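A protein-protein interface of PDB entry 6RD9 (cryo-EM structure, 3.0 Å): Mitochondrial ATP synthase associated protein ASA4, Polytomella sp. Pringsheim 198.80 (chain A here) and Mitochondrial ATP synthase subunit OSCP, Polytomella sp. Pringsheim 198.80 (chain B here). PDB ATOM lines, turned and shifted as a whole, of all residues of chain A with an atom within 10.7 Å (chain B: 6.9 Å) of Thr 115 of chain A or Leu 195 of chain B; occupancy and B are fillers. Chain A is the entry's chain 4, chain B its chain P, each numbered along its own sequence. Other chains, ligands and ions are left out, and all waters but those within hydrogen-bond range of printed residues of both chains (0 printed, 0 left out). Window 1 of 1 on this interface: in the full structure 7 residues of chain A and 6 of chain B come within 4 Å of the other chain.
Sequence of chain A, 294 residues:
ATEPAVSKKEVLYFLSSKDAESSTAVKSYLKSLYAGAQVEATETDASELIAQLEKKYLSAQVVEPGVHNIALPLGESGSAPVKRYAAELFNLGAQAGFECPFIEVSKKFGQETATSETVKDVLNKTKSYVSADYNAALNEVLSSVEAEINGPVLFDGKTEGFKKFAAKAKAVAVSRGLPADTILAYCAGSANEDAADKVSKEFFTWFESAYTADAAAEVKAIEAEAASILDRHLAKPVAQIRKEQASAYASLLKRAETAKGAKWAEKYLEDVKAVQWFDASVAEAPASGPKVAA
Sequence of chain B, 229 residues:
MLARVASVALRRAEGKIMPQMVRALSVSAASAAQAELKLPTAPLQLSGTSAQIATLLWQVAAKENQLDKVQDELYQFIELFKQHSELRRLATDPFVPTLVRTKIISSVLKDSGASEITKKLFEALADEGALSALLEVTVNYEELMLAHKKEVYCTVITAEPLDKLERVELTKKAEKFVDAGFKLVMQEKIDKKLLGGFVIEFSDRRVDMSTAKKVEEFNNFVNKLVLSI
O of Glu 117 of chain A sits at hydrogen-bond distance from N of Phe 155 of chain A, at 2.4 Å. The side-chain hydroxyl (OG) of Ser 116 of chain A lies within hydrogen-bond range of the side-chain carboxylate (OD1) of Asp 121 of chain A (2.9 Å).
Hydrophobic or aromatic side chains of chain B within 4 Å of the printed part of chain A: Leu 195. Of the 24 printed residues of chain A, 3 touch a printed residue of chain B. Among the printed residues, 5 pairs touch across the chains.
Ala 114 of chain A touches none of the printed residues of chain B. Printed residues of chain B within 4 Å of Ser 116 of chain A: Lys 193. Of the printed residues of chain B, Glu 117 of chain A touches Lys 193 (3.6 Å). Of the printed residues of chain A, Lys 192 of chain B touches Thr 115 (3.9 Å). Of the printed residues of chain A, Leu 195 of chain B touches Thr 115. No residue of chain A comes within 4 Å of Gly 196 of chain B. No residue of chain A comes within 4 Å of Thr 211 of chain B. Val 215 of chain B touches none of the printed residues of chain A. The nearest residue of chain B that does not touch Thr 115 of chain A is Leu 194 of chain B (5.3 Å). The nearest printed residue of chain A that does not touch Lys 192 of chain B is Glu 117 of chain A (4.4 Å).
Among the printed residues, merely in contact across the chains: Thr 115 of chain A with Leu 195 of chain B, Ser 116 of chain A with Lys 193 of chain B and Thr 115 of chain A with Lys 192 of chain B.
O of Thr 115 of chain A is in hydrogen-bond range of NZ of Lys 193 of chain B (2.8 Å). OE1 of Glu 117 of chain A lies within salt-bridge range of NZ of Lys 193 of chain B (3.7 Å).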
ATOM      1  N   GLU A  48       0.284   7.157   6.397  1.00  0.00           N
ATOM      2  CA  GLU A  48      -1.091   6.655   6.372  1.00  0.00           C
ATOM      3  C   GLU A  48      -1.575   6.066   5.053  1.00  0.00           C
ATOM      4  O   GLU A  48      -2.259   5.042   5.049  1.00  0.00           O
ATOM      5  CB  GLU A  48      -2.033   7.784   6.795  1.00  0.00           C
ATOM      6  CG  GLU A  48      -3.500   7.397   6.912  1.00  0.00           C
ATOM      7  CD  GLU A  48      -3.778   6.420   8.047  1.00  0.00           C
ATOM      8  OE1 GLU A  48      -3.029   6.420   9.047  1.00  0.00           O
ATOM      9  OE2 GLU A  48      -4.753   5.648   7.940  1.00  0.00           O
ATOM     10  N   LEU A  49      -1.210   6.677   3.927  1.00  0.00           N
ATOM     11  CA  LEU A  49      -1.615   6.125   2.641  1.00  0.00           C
ATOM     12  C   LEU A  49      -0.841   4.863   2.294  1.00  0.00           C
ATOM     13  O   LEU A  49      -1.384   3.970   1.641  1.00  0.00           O
ATOM     14  CB  LEU A  49      -1.436   7.164   1.541  1.00  0.00           C
ATOM     15  CG  LEU A  49      -2.426   8.322   1.518  1.00  0.00           C
ATOM     16  CD1 LEU A  49      -2.068   9.280   0.403  1.00  0.00           C
ATOM     17  CD2 LEU A  49      -3.838   7.805   1.350  1.00  0.00           C
ATOM     18  N   GLN A  52      -2.230   2.027   4.659  1.00  0.00           N
ATOM     19  CA  GLN A  52      -3.490   1.484   4.180  1.00  0.00           C
ATOM     20  C   GLN A  52      -3.291   0.619   2.951  1.00  0.00           C
ATOM     21  O   GLN A  52      -4.089  -0.283   2.696  1.00  0.00           O
ATOM     22  CB  GLN A  52      -4.463   2.605   3.850  1.00  0.00           C
ATOM     23  CG  GLN A  52      -5.028   3.325   5.037  1.00  0.00           C
ATOM     24  CD  GLN A  52      -5.917   4.472   4.615  1.00  0.00           C
ATOM     25  OE1 GLN A  52      -5.970   5.509   5.274  1.00  0.00           O
ATOM     26  NE2 GLN A  52      -6.625   4.290   3.507  1.00  0.00           N
ATOM     27  N   LYS A 108     -16.307   2.407   5.238  1.00  0.00           N
ATOM     28  CA  LYS A 108     -16.178   2.749   3.826  1.00  0.00           C
ATOM     29  C   LYS A 108     -17.106   3.884   3.435  1.00  0.00           C
ATOM     30  O   LYS A 108     -16.789   4.648   2.521  1.00  0.00           O
ATOM     31  CB  LYS A 108     -16.464   1.535   2.953  1.00  0.00           C
ATOM     32  CG  LYS A 108     -15.737   1.570   1.639  1.00  0.00           C
ATOM     33  CD  LYS A 108     -14.297   1.240   1.854  1.00  0.00           C
ATOM     34  CE  LYS A 108     -13.565   1.148   0.556  1.00  0.00           C
ATOM     35  NZ  LYS A 108     -12.197   0.628   0.792  1.00  0.00           N
ATOM     36  N   PHE A 109     -18.250   4.006   4.101  1.00  0.00           N
ATOM     37  CA  PHE A 109     -19.150   5.111   3.808  1.00  0.00           C
ATOM     38  C   PHE A 109     -18.562   6.426   4.287  1.00  0.00           C
ATOM     39  O   PHE A 109     -18.383   7.360   3.500  1.00  0.00           O
ATOM     40  CB  PHE A 109     -20.500   4.875   4.464  1.00  0.00           C
ATOM     41  CG  PHE A 109     -21.278   3.764   3.868  1.00  0.00           C
ATOM     42  CD1 PHE A 109     -21.160   3.457   2.540  1.00  0.00           C
ATOM     43  CD2 PHE A 109     -22.148   3.033   4.639  1.00  0.00           C
ATOM     44  CE1 PHE A 109     -21.891   2.441   1.998  1.00  0.00           C
ATOM     45  CE2 PHE A 109     -22.872   2.018   4.096  1.00  0.00           C
ATOM     46  CZ  PHE A 109     -22.743   1.723   2.774  1.00  0.00           C
ATOM     47  N   GLY A 110     -18.210   6.500   5.570  1.00  0.00           N
ATOM     48  CA  GLY A 110     -17.714   7.732   6.149  1.00  0.00           C
ATOM     49  C   GLY A 110     -16.350   8.148   5.659  1.00  0.00           C
ATOM     50  O   GLY A 110     -15.956   9.295   5.872  1.00  0.00           O
ATOM     51  N   GLN A 111     -15.613   7.248   5.025  1.00  0.00           N
ATOM     52  CA  GLN A 111     -14.364   7.639   4.392  1.00  0.00           C
ATOM     53  C   GLN A 111     -14.610   8.212   3.006  1.00  0.00           C
ATOM     54  O   GLN A 111     -13.963   9.185   2.610  1.00  0.00           O
ATOM     55  CB  GLN A 111     -13.421   6.441   4.331  1.00  0.00           C
ATOM     56  CG  GLN A 111     -12.266   6.553   3.379  1.00  0.00           C
ATOM     57  CD  GLN A 111     -11.646   5.208   3.098  1.00  0.00           C
ATOM     58  OE1 GLN A 111     -11.537   4.368   3.989  1.00  0.00           O
ATOM     59  NE2 GLN A 111     -11.253   4.986   1.852  1.00  0.00           N
ATOM     60  N   GLU A 112     -15.552   7.636   2.263  1.00  0.00           N
ATOM     61  CA  GLU A 112     -15.817   8.126   0.916  1.00  0.00           C
ATOM     62  C   GLU A 112     -16.577   9.443   0.933  1.00  0.00           C
ATOM     63  O   GLU A 112     -16.478  10.221  -0.019  1.00  0.00           O
ATOM     64  CB  GLU A 112     -16.594   7.083   0.113  1.00  0.00           C
ATOM     65  CG  GLU A 112     -15.767   5.902  -0.346  1.00  0.00           C
ATOM     66  CD  GLU A 112     -14.768   6.265  -1.419  1.00  0.00           C
ATOM     67  OE1 GLU A 112     -15.039   7.203  -2.195  1.00  0.00           O
ATOM     68  OE2 GLU A 112     -13.709   5.608  -1.492  1.00  0.00           O
ATOM     69  N   THR A 113     -17.322   9.718   1.998  1.00  0.00           N
ATOM     70  CA  THR A 113     -18.110  10.938   2.084  1.00  0.00           C
ATOM     71  C   THR A 113     -17.657  11.829   3.229  1.00  0.00           C
ATOM     72  O   THR A 113     -18.489  12.330   3.990  1.00  0.00           O
ATOM     73  CB  THR A 113     -19.584  10.610   2.262  1.00  0.00           C
ATOM     74  OG1 THR A 113     -19.732   9.731   3.372  1.00  0.00           O
ATOM     75  CG2 THR A 113     -20.120   9.937   1.042  1.00  0.00           C
ATOM     76  N   ALA A 114     -16.353  12.019   3.388  1.00  0.00           N
ATOM     77  CA  ALA A 114     -15.877  12.939   4.410  1.00  0.00           C
ATOM     78  C   ALA A 114     -15.908  14.390   3.953  1.00  0.00           C
ATOM     79  O   ALA A 114     -15.708  15.290   4.776  1.00  0.00           O
ATOM     80  CB  ALA A 114     -14.458  12.570   4.837  1.00  0.00           C
ATOM     81  N   THR A 115     -16.161  14.636   2.671  1.00  0.00           N
ATOM     82  CA  THR A 115     -16.137  15.970   2.094  1.00  0.00           C
ATOM     83  C   THR A 115     -17.531  16.508   1.827  1.00  0.00           C
ATOM     84  O   THR A 115     -17.673  17.663   1.421  1.00  0.00           O
ATOM     85  CB  THR A 115     -15.349  15.960   0.786  1.00  0.00           C
ATOM     86  OG1 THR A 115     -15.919  14.989  -0.100  1.00  0.00           O
ATOM     87  CG2 THR A 115     -13.912  15.592   1.044  1.00  0.00           C
ATOM     88  N   SER A 116     -18.560  15.703   2.037  1.00  0.00           N
ATOM     89  CA  SER A 116     -19.888  15.991   1.528  1.00  0.00           C
ATOM     90  C   SER A 116     -20.749  16.587   2.627  1.00  0.00           C
ATOM     91  O   SER A 116     -20.736  16.104   3.763  1.00  0.00           O
ATOM     92  CB  SER A 116     -20.536  14.723   0.979  1.00  0.00           C
ATOM     93  OG  SER A 116     -19.642  14.030   0.127  1.00  0.00           O
ATOM     94  N   GLU A 117     -21.484  17.641   2.285  1.00  0.00           N
ATOM     95  CA  GLU A 117     -22.483  18.196   3.187  1.00  0.00           C
ATOM     96  C   GLU A 117     -23.866  18.225   2.556  1.00  0.00           C
ATOM     97  O   GLU A 117     -24.819  18.668   3.208  1.00  0.00           O
ATOM     98  CB  GLU A 117     -22.084  19.602   3.654  1.00  0.00           C
ATOM     99  CG  GLU A 117     -21.851  20.597   2.534  1.00  0.00           C
ATOM    100  CD  GLU A 117     -20.383  20.688   2.144  1.00  0.00           C
ATOM    101  OE1 GLU A 117     -19.589  19.841   2.599  1.00  0.00           O
ATOM    102  OE2 GLU A 117     -20.024  21.601   1.375  1.00  0.00           O
ATOM    103  N   THR A 118     -24.011  17.754   1.327  1.00  0.00           N
ATOM    104  CA  THR A 118     -25.307  17.575   0.701  1.00  0.00           C
ATOM    105  C   THR A 118     -25.588  16.095   0.491  1.00  0.00           C
ATOM    106  O   THR A 118     -24.674  15.293   0.292  1.00  0.00           O
ATOM    107  CB  THR A 118     -25.382  18.313  -0.631  1.00  0.00           C
ATOM    108  OG1 THR A 118     -26.556  17.895  -1.333  1.00  0.00           O
ATOM    109  CG2 THR A 118     -24.148  18.044  -1.464  1.00  0.00           C
ATOM    110  N   VAL A 119     -26.871  15.747   0.530  1.00  0.00           N
ATOM    111  CA  VAL A 119     -27.271  14.348   0.478  1.00  0.00           C
ATOM    112  C   VAL A 119     -27.138  13.792  -0.932  1.00  0.00           C
ATOM    113  O   VAL A 119     -26.777  12.625  -1.109  1.00  0.00           O
ATOM    114  CB  VAL A 119     -28.696  14.227   1.042  1.00  0.00           C
ATOM    115  CG1 VAL A 119     -29.257  12.853   0.869  1.00  0.00           C
ATOM    116  CG2 VAL A 119     -28.674  14.560   2.506  1.00  0.00           C
ATOM    117  N   LYS A 120     -27.339  14.626  -1.954  1.00  0.00           N
ATOM    118  CA  LYS A 120     -27.230  14.162  -3.333  1.00  0.00           C
ATOM    119  C   LYS A 120     -25.798  13.808  -3.694  1.00  0.00           C
ATOM    120  O   LYS A 120     -25.573  13.044  -4.630  1.00  0.00           O
ATOM    121  CB  LYS A 120     -27.768  15.226  -4.289  1.00  0.00           C
ATOM    122  CG  LYS A 120     -28.229  14.705  -5.649  1.00  0.00           C
ATOM    123  CD  LYS A 120     -27.185  14.889  -6.744  1.00  0.00           C
ATOM    124  CE  LYS A 120     -26.989  16.340  -7.099  1.00  0.00           C
ATOM    125  NZ  LYS A 120     -25.975  16.487  -8.171  1.00  0.00           N
ATOM    126  N   ASP A 121     -24.823  14.337  -2.969  1.00  0.00           N
ATOM    127  CA  ASP A 121     -23.454  13.892  -3.172  1.00  0.00           C
ATOM    128  C   ASP A 121     -23.127  12.691  -2.298  1.00  0.00           C
ATOM    129  O   ASP A 121     -22.287  11.872  -2.675  1.00  0.00           O
ATOM    130  CB  ASP A 121     -22.502  15.059  -2.918  1.00  0.00           C
ATOM    131  CG  ASP A 121     -21.082  14.767  -3.333  1.00  0.00           C
ATOM    132  OD1 ASP A 121     -20.389  13.991  -2.654  1.00  0.00           O
ATOM    133  OD2 ASP A 121     -20.656  15.315  -4.366  1.00  0.00           O
ATOM    134  N   VAL A 122     -23.781  12.559  -1.144  1.00  0.00           N
ATOM    135  CA  VAL A 122     -23.607  11.368  -0.318  1.00  0.00           C
ATOM    136  C   VAL A 122     -24.186  10.148  -1.019  1.00  0.00           C
ATOM    137  O   VAL A 122     -23.540   9.102  -1.113  1.00  0.00           O
ATOM    138  CB  VAL A 122     -24.244  11.583   1.064  1.00  0.00           C
ATOM    139  CG1 VAL A 122     -24.435  10.279   1.788  1.00  0.00           C
ATOM    140  CG2 VAL A 122     -23.379  12.496   1.871  1.00  0.00           C
ATOM    141  N   LEU A 123     -25.370  10.292  -1.601  1.00  0.00           N
ATOM    142  CA  LEU A 123     -25.979   9.242  -2.404  1.00  0.00           C
ATOM    143  C   LEU A 123     -25.305   9.038  -3.749  1.00  0.00           C
ATOM    144  O   LEU A 123     -25.821   8.262  -4.549  1.00  0.00           O
ATOM    145  CB  LEU A 123     -27.458   9.544  -2.640  1.00  0.00           C
ATOM    146  CG  LEU A 123     -28.547   9.043  -1.695  1.00  0.00           C
ATOM    147  CD1 LEU A 123     -28.612   7.563  -1.763  1.00  0.00           C
ATOM    148  CD2 LEU A 123     -28.309   9.445  -0.275  1.00  0.00           C
ATOM    149  N   ASN A 124     -24.196   9.711  -4.047  1.00  0.00           N
ATOM    150  CA  ASN A 124     -23.589   9.609  -5.358  1.00  0.00           C
ATOM    151  C   ASN A 124     -22.187   9.032  -5.330  1.00  0.00           C
ATOM    152  O   ASN A 124     -21.782   8.407  -6.312  1.00  0.00           O
ATOM    153  CB  ASN A 124     -23.544  10.985  -6.027  1.00  0.00           C
ATOM    154  CG  ASN A 124     -23.491  10.907  -7.526  1.00  0.00           C
ATOM    155  OD1 ASN A 124     -23.509   9.830  -8.109  1.00  0.00           O
ATOM    156  ND2 ASN A 124     -23.442  12.062  -8.166  1.00  0.00           N
ATOM    157  N   LYS A 125     -21.431   9.224  -4.253  1.00  0.00           N
ATOM    158  CA  LYS A 125     -20.135   8.572  -4.131  1.00  0.00           C
ATOM    159  C   LYS A 125     -20.147   7.437  -3.118  1.00  0.00           C
ATOM    160  O   LYS A 125     -19.102   6.834  -2.869  1.00  0.00           O
ATOM    161  CB  LYS A 125     -19.037   9.578  -3.792  1.00  0.00           C
ATOM    162  CG  LYS A 125     -19.341  10.503  -2.649  1.00  0.00           C
ATOM    163  CD  LYS A 125     -18.232  11.518  -2.449  1.00  0.00           C
ATOM    164  CE  LYS A 125     -17.814  12.184  -3.748  1.00  0.00           C
ATOM    165  NZ  LYS A 125     -16.900  13.334  -3.521  1.00  0.00           N
ATOM    166  N   THR A 126     -21.300   7.138  -2.522  1.00  0.00           N
ATOM    167  CA  THR A 126     -21.561   5.822  -1.958  1.00  0.00           C
ATOM    168  C   THR A 126     -22.394   4.981  -2.902  1.00  0.00           C
ATOM    169  O   THR A 126     -23.247   4.213  -2.463  1.00  0.00           O
ATOM    170  CB  THR A 126     -22.259   5.908  -0.606  1.00  0.00           C
ATOM    171  OG1 THR A 126     -23.437   6.701  -0.722  1.00  0.00           O
ATOM    172  CG2 THR A 126     -21.353   6.498   0.422  1.00  0.00           C
ATOM    173  N   LEU A 154     -29.469  18.990   2.904  1.00  0.00           N
ATOM    174  CA  LEU A 154     -28.132  19.023   3.460  1.00  0.00           C
ATOM    175  C   LEU A 154     -27.856  17.784   4.293  1.00  0.00           C
ATOM    176  O   LEU A 154     -28.765  17.188   4.877  1.00  0.00           O
ATOM    177  CB  LEU A 154     -27.935  20.274   4.313  1.00  0.00           C
ATOM    178  CG  LEU A 154     -27.924  21.602   3.566  1.00  0.00           C
ATOM    179  CD1 LEU A 154     -27.490  22.699   4.511  1.00  0.00           C
ATOM    180  CD2 LEU A 154     -27.028  21.550   2.337  1.00  0.00           C
ATOM    181  N   PHE A 155     -26.582  17.406   4.341  1.00  0.00           N
ATOM    182  CA  PHE A 155     -26.110  16.346   5.227  1.00  0.00           C
ATOM    183  C   PHE A 155     -25.705  16.996   6.551  1.00  0.00           C
ATOM    184  O   PHE A 155     -24.530  17.164   6.876  1.00  0.00           O
ATOM    185  CB  PHE A 155     -24.960  15.599   4.564  1.00  0.00           C
ATOM    186  CG  PHE A 155     -24.780  14.196   5.047  1.00  0.00           C
ATOM    187  CD1 PHE A 155     -25.873  13.374   5.253  1.00  0.00           C
ATOM    188  CD2 PHE A 155     -23.510  13.684   5.252  1.00  0.00           C
ATOM    189  CE1 PHE A 155     -25.703  12.083   5.684  1.00  0.00           C
ATOM    190  CE2 PHE A 155     -23.336  12.390   5.667  1.00  0.00           C
ATOM    191  CZ  PHE A 155     -24.436  11.594   5.897  1.00  0.00           C
ATOM    192  N   ALA B 159      -8.468  23.922   4.757  1.00  0.00           N
ATOM    193  CA  ALA B 159      -9.615  23.105   5.135  1.00  0.00           C
ATOM    194  C   ALA B 159     -10.417  23.755   6.259  1.00  0.00           C
ATOM    195  O   ALA B 159     -11.640  23.897   6.165  1.00  0.00           O
ATOM    196  CB  ALA B 159      -9.143  21.703   5.528  1.00  0.00           C
ATOM    197  N   GLU B 160      -9.745  24.138   7.334  1.00  0.00           N
ATOM    198  CA  GLU B 160     -10.312  24.913   8.424  1.00  0.00           C
ATOM    199  C   GLU B 160      -9.416  26.124   8.631  1.00  0.00           C
ATOM    200  O   GLU B 160      -8.284  26.140   8.135  1.00  0.00           O
ATOM    201  CB  GLU B 160     -10.416  24.062   9.703  1.00  0.00           C
ATOM    202  CG  GLU B 160      -9.097  23.697  10.346  1.00  0.00           C
ATOM    203  CD  GLU B 160      -8.553  22.373   9.858  1.00  0.00           C
ATOM    204  OE1 GLU B 160      -9.034  21.867   8.828  1.00  0.00           O
ATOM    205  OE2 GLU B 160      -7.644  21.827  10.515  1.00  0.00           O
ATOM    206  N   ASP B 191     -12.127  25.526   2.651  1.00  0.00           N
ATOM    207  CA  ASP B 191     -12.875  24.521   1.887  1.00  0.00           C
ATOM    208  C   ASP B 191     -12.584  23.149   2.493  1.00  0.00           C
ATOM    209  O   ASP B 191     -11.466  22.648   2.369  1.00  0.00           O
ATOM    210  CB  ASP B 191     -12.506  24.549   0.417  1.00  0.00           C
ATOM    211  CG  ASP B 191     -13.639  24.091  -0.474  1.00  0.00           C
ATOM    212  OD1 ASP B 191     -13.473  24.128  -1.709  1.00  0.00           O
ATOM    213  OD2 ASP B 191     -14.694  23.683   0.059  1.00  0.00           O
ATOM    214  N   LYS B 192     -13.592  22.547   3.119  1.00  0.00           N
ATOM    215  CA  LYS B 192     -13.427  21.199   3.645  1.00  0.00           C
ATOM    216  C   LYS B 192     -13.597  20.113   2.591  1.00  0.00           C
ATOM    217  O   LYS B 192     -13.509  18.929   2.928  1.00  0.00           O
ATOM    218  CB  LYS B 192     -14.385  20.967   4.809  1.00  0.00           C
ATOM    219  CG  LYS B 192     -15.837  21.231   4.501  1.00  0.00           C
ATOM    220  CD  LYS B 192     -16.685  20.880   5.709  1.00  0.00           C
ATOM    221  CE  LYS B 192     -16.325  21.748   6.908  1.00  0.00           C
ATOM    222  NZ  LYS B 192     -16.590  23.190   6.689  1.00  0.00           N
ATOM    223  N   LYS B 193     -13.823  20.479   1.328  1.00  0.00           N
ATOM    224  CA  LYS B 193     -13.582  19.544   0.238  1.00  0.00           C
ATOM    225  C   LYS B 193     -12.101  19.202   0.129  1.00  0.00           C
ATOM    226  O   LYS B 193     -11.743  18.152  -0.410  1.00  0.00           O
ATOM    227  CB  LYS B 193     -14.097  20.126  -1.075  1.00  0.00           C
ATOM    228  CG  LYS B 193     -15.542  20.596  -1.027  1.00  0.00           C
ATOM    229  CD  LYS B 193     -16.521  19.451  -1.231  1.00  0.00           C
ATOM    230  CE  LYS B 193     -17.953  19.917  -1.004  1.00  0.00           C
ATOM    231  NZ  LYS B 193     -18.917  18.787  -0.876  1.00  0.00           N
ATOM    232  N   LEU B 194     -11.234  20.095   0.591  1.00  0.00           N
ATOM    233  CA  LEU B 194      -9.846  19.754   0.844  1.00  0.00           C
ATOM    234  C   LEU B 194      -9.744  19.044   2.185  1.00  0.00           C
ATOM    235  O   LEU B 194     -10.394  19.438   3.155  1.00  0.00           O
ATOM    236  CB  LEU B 194      -8.987  21.014   0.860  1.00  0.00           C
ATOM    237  CG  LEU B 194      -8.374  21.638  -0.390  1.00  0.00           C
ATOM    238  CD1 LEU B 194      -9.408  22.025  -1.430  1.00  0.00           C
ATOM    239  CD2 LEU B 194      -7.591  22.854   0.038  1.00  0.00           C
ATOM    240  N   LEU B 195      -8.954  17.982   2.237  1.00  0.00           N
ATOM    241  CA  LEU B 195      -8.675  17.289   3.494  1.00  0.00           C
ATOM    242  C   LEU B 195      -7.315  17.695   4.045  1.00  0.00           C
ATOM    243  O   LEU B 195      -6.419  16.878   4.228  1.00  0.00           O
ATOM    244  CB  LEU B 195      -8.754  15.781   3.300  1.00  0.00           C
ATOM    245  CG  LEU B 195      -9.984  15.270   2.578  1.00  0.00           C
ATOM    246  CD1 LEU B 195      -9.846  13.796   2.310  1.00  0.00           C
ATOM    247  CD2 LEU B 195     -11.157  15.538   3.477  1.00  0.00           C
ATOM    248  N   GLY B 196      -7.161  18.978   4.313  1.00  0.00           N
ATOM    249  CA  GLY B 196      -5.899  19.463   4.819  1.00  0.00           C
ATOM    250  C   GLY B 196      -4.891  19.703   3.710  1.00  0.00           C
ATOM    251  O   GLY B 196      -5.051  19.264   2.574  1.00  0.00           O
ATOM    252  N   GLY B 197      -3.821  20.399   4.068  1.00  0.00           N
ATOM    253  CA  GLY B 197      -2.948  20.963   3.065  1.00  0.00           C
ATOM    254  C   GLY B 197      -3.524  22.298   2.654  1.00  0.00           C
ATOM    255  O   GLY B 197      -4.281  22.899   3.420  1.00  0.00           O
ATOM    256  N   SER B 210      -2.565  20.363  -1.326  1.00  0.00           N
ATOM    257  CA  SER B 210      -3.585  19.821  -0.453  1.00  0.00           C
ATOM    258  C   SER B 210      -3.545  18.306  -0.489  1.00  0.00           C
ATOM    259  O   SER B 210      -3.192  17.701  -1.500  1.00  0.00           O
ATOM    260  CB  SER B 210      -4.964  20.302  -0.880  1.00  0.00           C
ATOM    261  OG  SER B 210      -5.336  19.723  -2.113  1.00  0.00           O
ATOM    262  N   THR B 211      -3.922  17.686   0.628  1.00  0.00           N
ATOM    263  CA  THR B 211      -3.904  16.235   0.684  1.00  0.00           C
ATOM    264  C   THR B 211      -5.138  15.611   0.061  1.00  0.00           C
ATOM    265  O   THR B 211      -5.168  14.395  -0.112  1.00  0.00           O
ATOM    266  CB  THR B 211      -3.757  15.736   2.123  1.00  0.00           C
ATOM    267  OG1 THR B 211      -5.029  15.770   2.778  1.00  0.00           O
ATOM    268  CG2 THR B 211      -2.768  16.592   2.888  1.00  0.00           C
ATOM    269  N   ALA B 212      -6.159  16.403  -0.264  1.00  0.00           N
ATOM    270  CA  ALA B 212      -7.300  15.854  -0.984  1.00  0.00           C
ATOM    271  C   ALA B 212      -6.922  15.482  -2.405  1.00  0.00           C
ATOM    272  O   ALA B 212      -7.475  14.534  -2.969  1.00  0.00           O
ATOM    273  CB  ALA B 212      -8.459  16.838  -0.988  1.00  0.00           C
ATOM    274  N   LYS B 213      -6.014  16.238  -3.017  1.00  0.00           N
ATOM    275  CA  LYS B 213      -5.481  15.829  -4.308  1.00  0.00           C
ATOM    276  C   LYS B 213      -4.305  14.876  -4.164  1.00  0.00           C
ATOM    277  O   LYS B 213      -4.037  14.098  -5.082  1.00  0.00           O
ATOM    278  CB  LYS B 213      -5.064  17.049  -5.130  1.00  0.00           C
ATOM    279  CG  LYS B 213      -4.969  16.773  -6.622  1.00  0.00           C
ATOM    280  CD  LYS B 213      -4.484  17.972  -7.383  1.00  0.00           C
ATOM    281  CE  LYS B 213      -2.995  18.129  -7.212  1.00  0.00           C
ATOM    282  NZ  LYS B 213      -2.256  17.017  -7.853  1.00  0.00           N
ATOM    283  N   VAL B 215      -4.332  12.407  -2.206  1.00  0.00           N
ATOM    284  CA  VAL B 215      -5.020  11.122  -2.245  1.00  0.00           C
ATOM    285  C   VAL B 215      -5.217  10.671  -3.685  1.00  0.00           C
ATOM    286  O   VAL B 215      -4.837   9.556  -4.056  1.00  0.00           O
ATOM    287  CB  VAL B 215      -6.361  11.214  -1.498  1.00  0.00           C
ATOM    288  CG1 VAL B 215      -7.204  10.007  -1.784  1.00  0.00           C
ATOM    289  CG2 VAL B 215      -6.118  11.299  -0.019  1.00  0.00           C
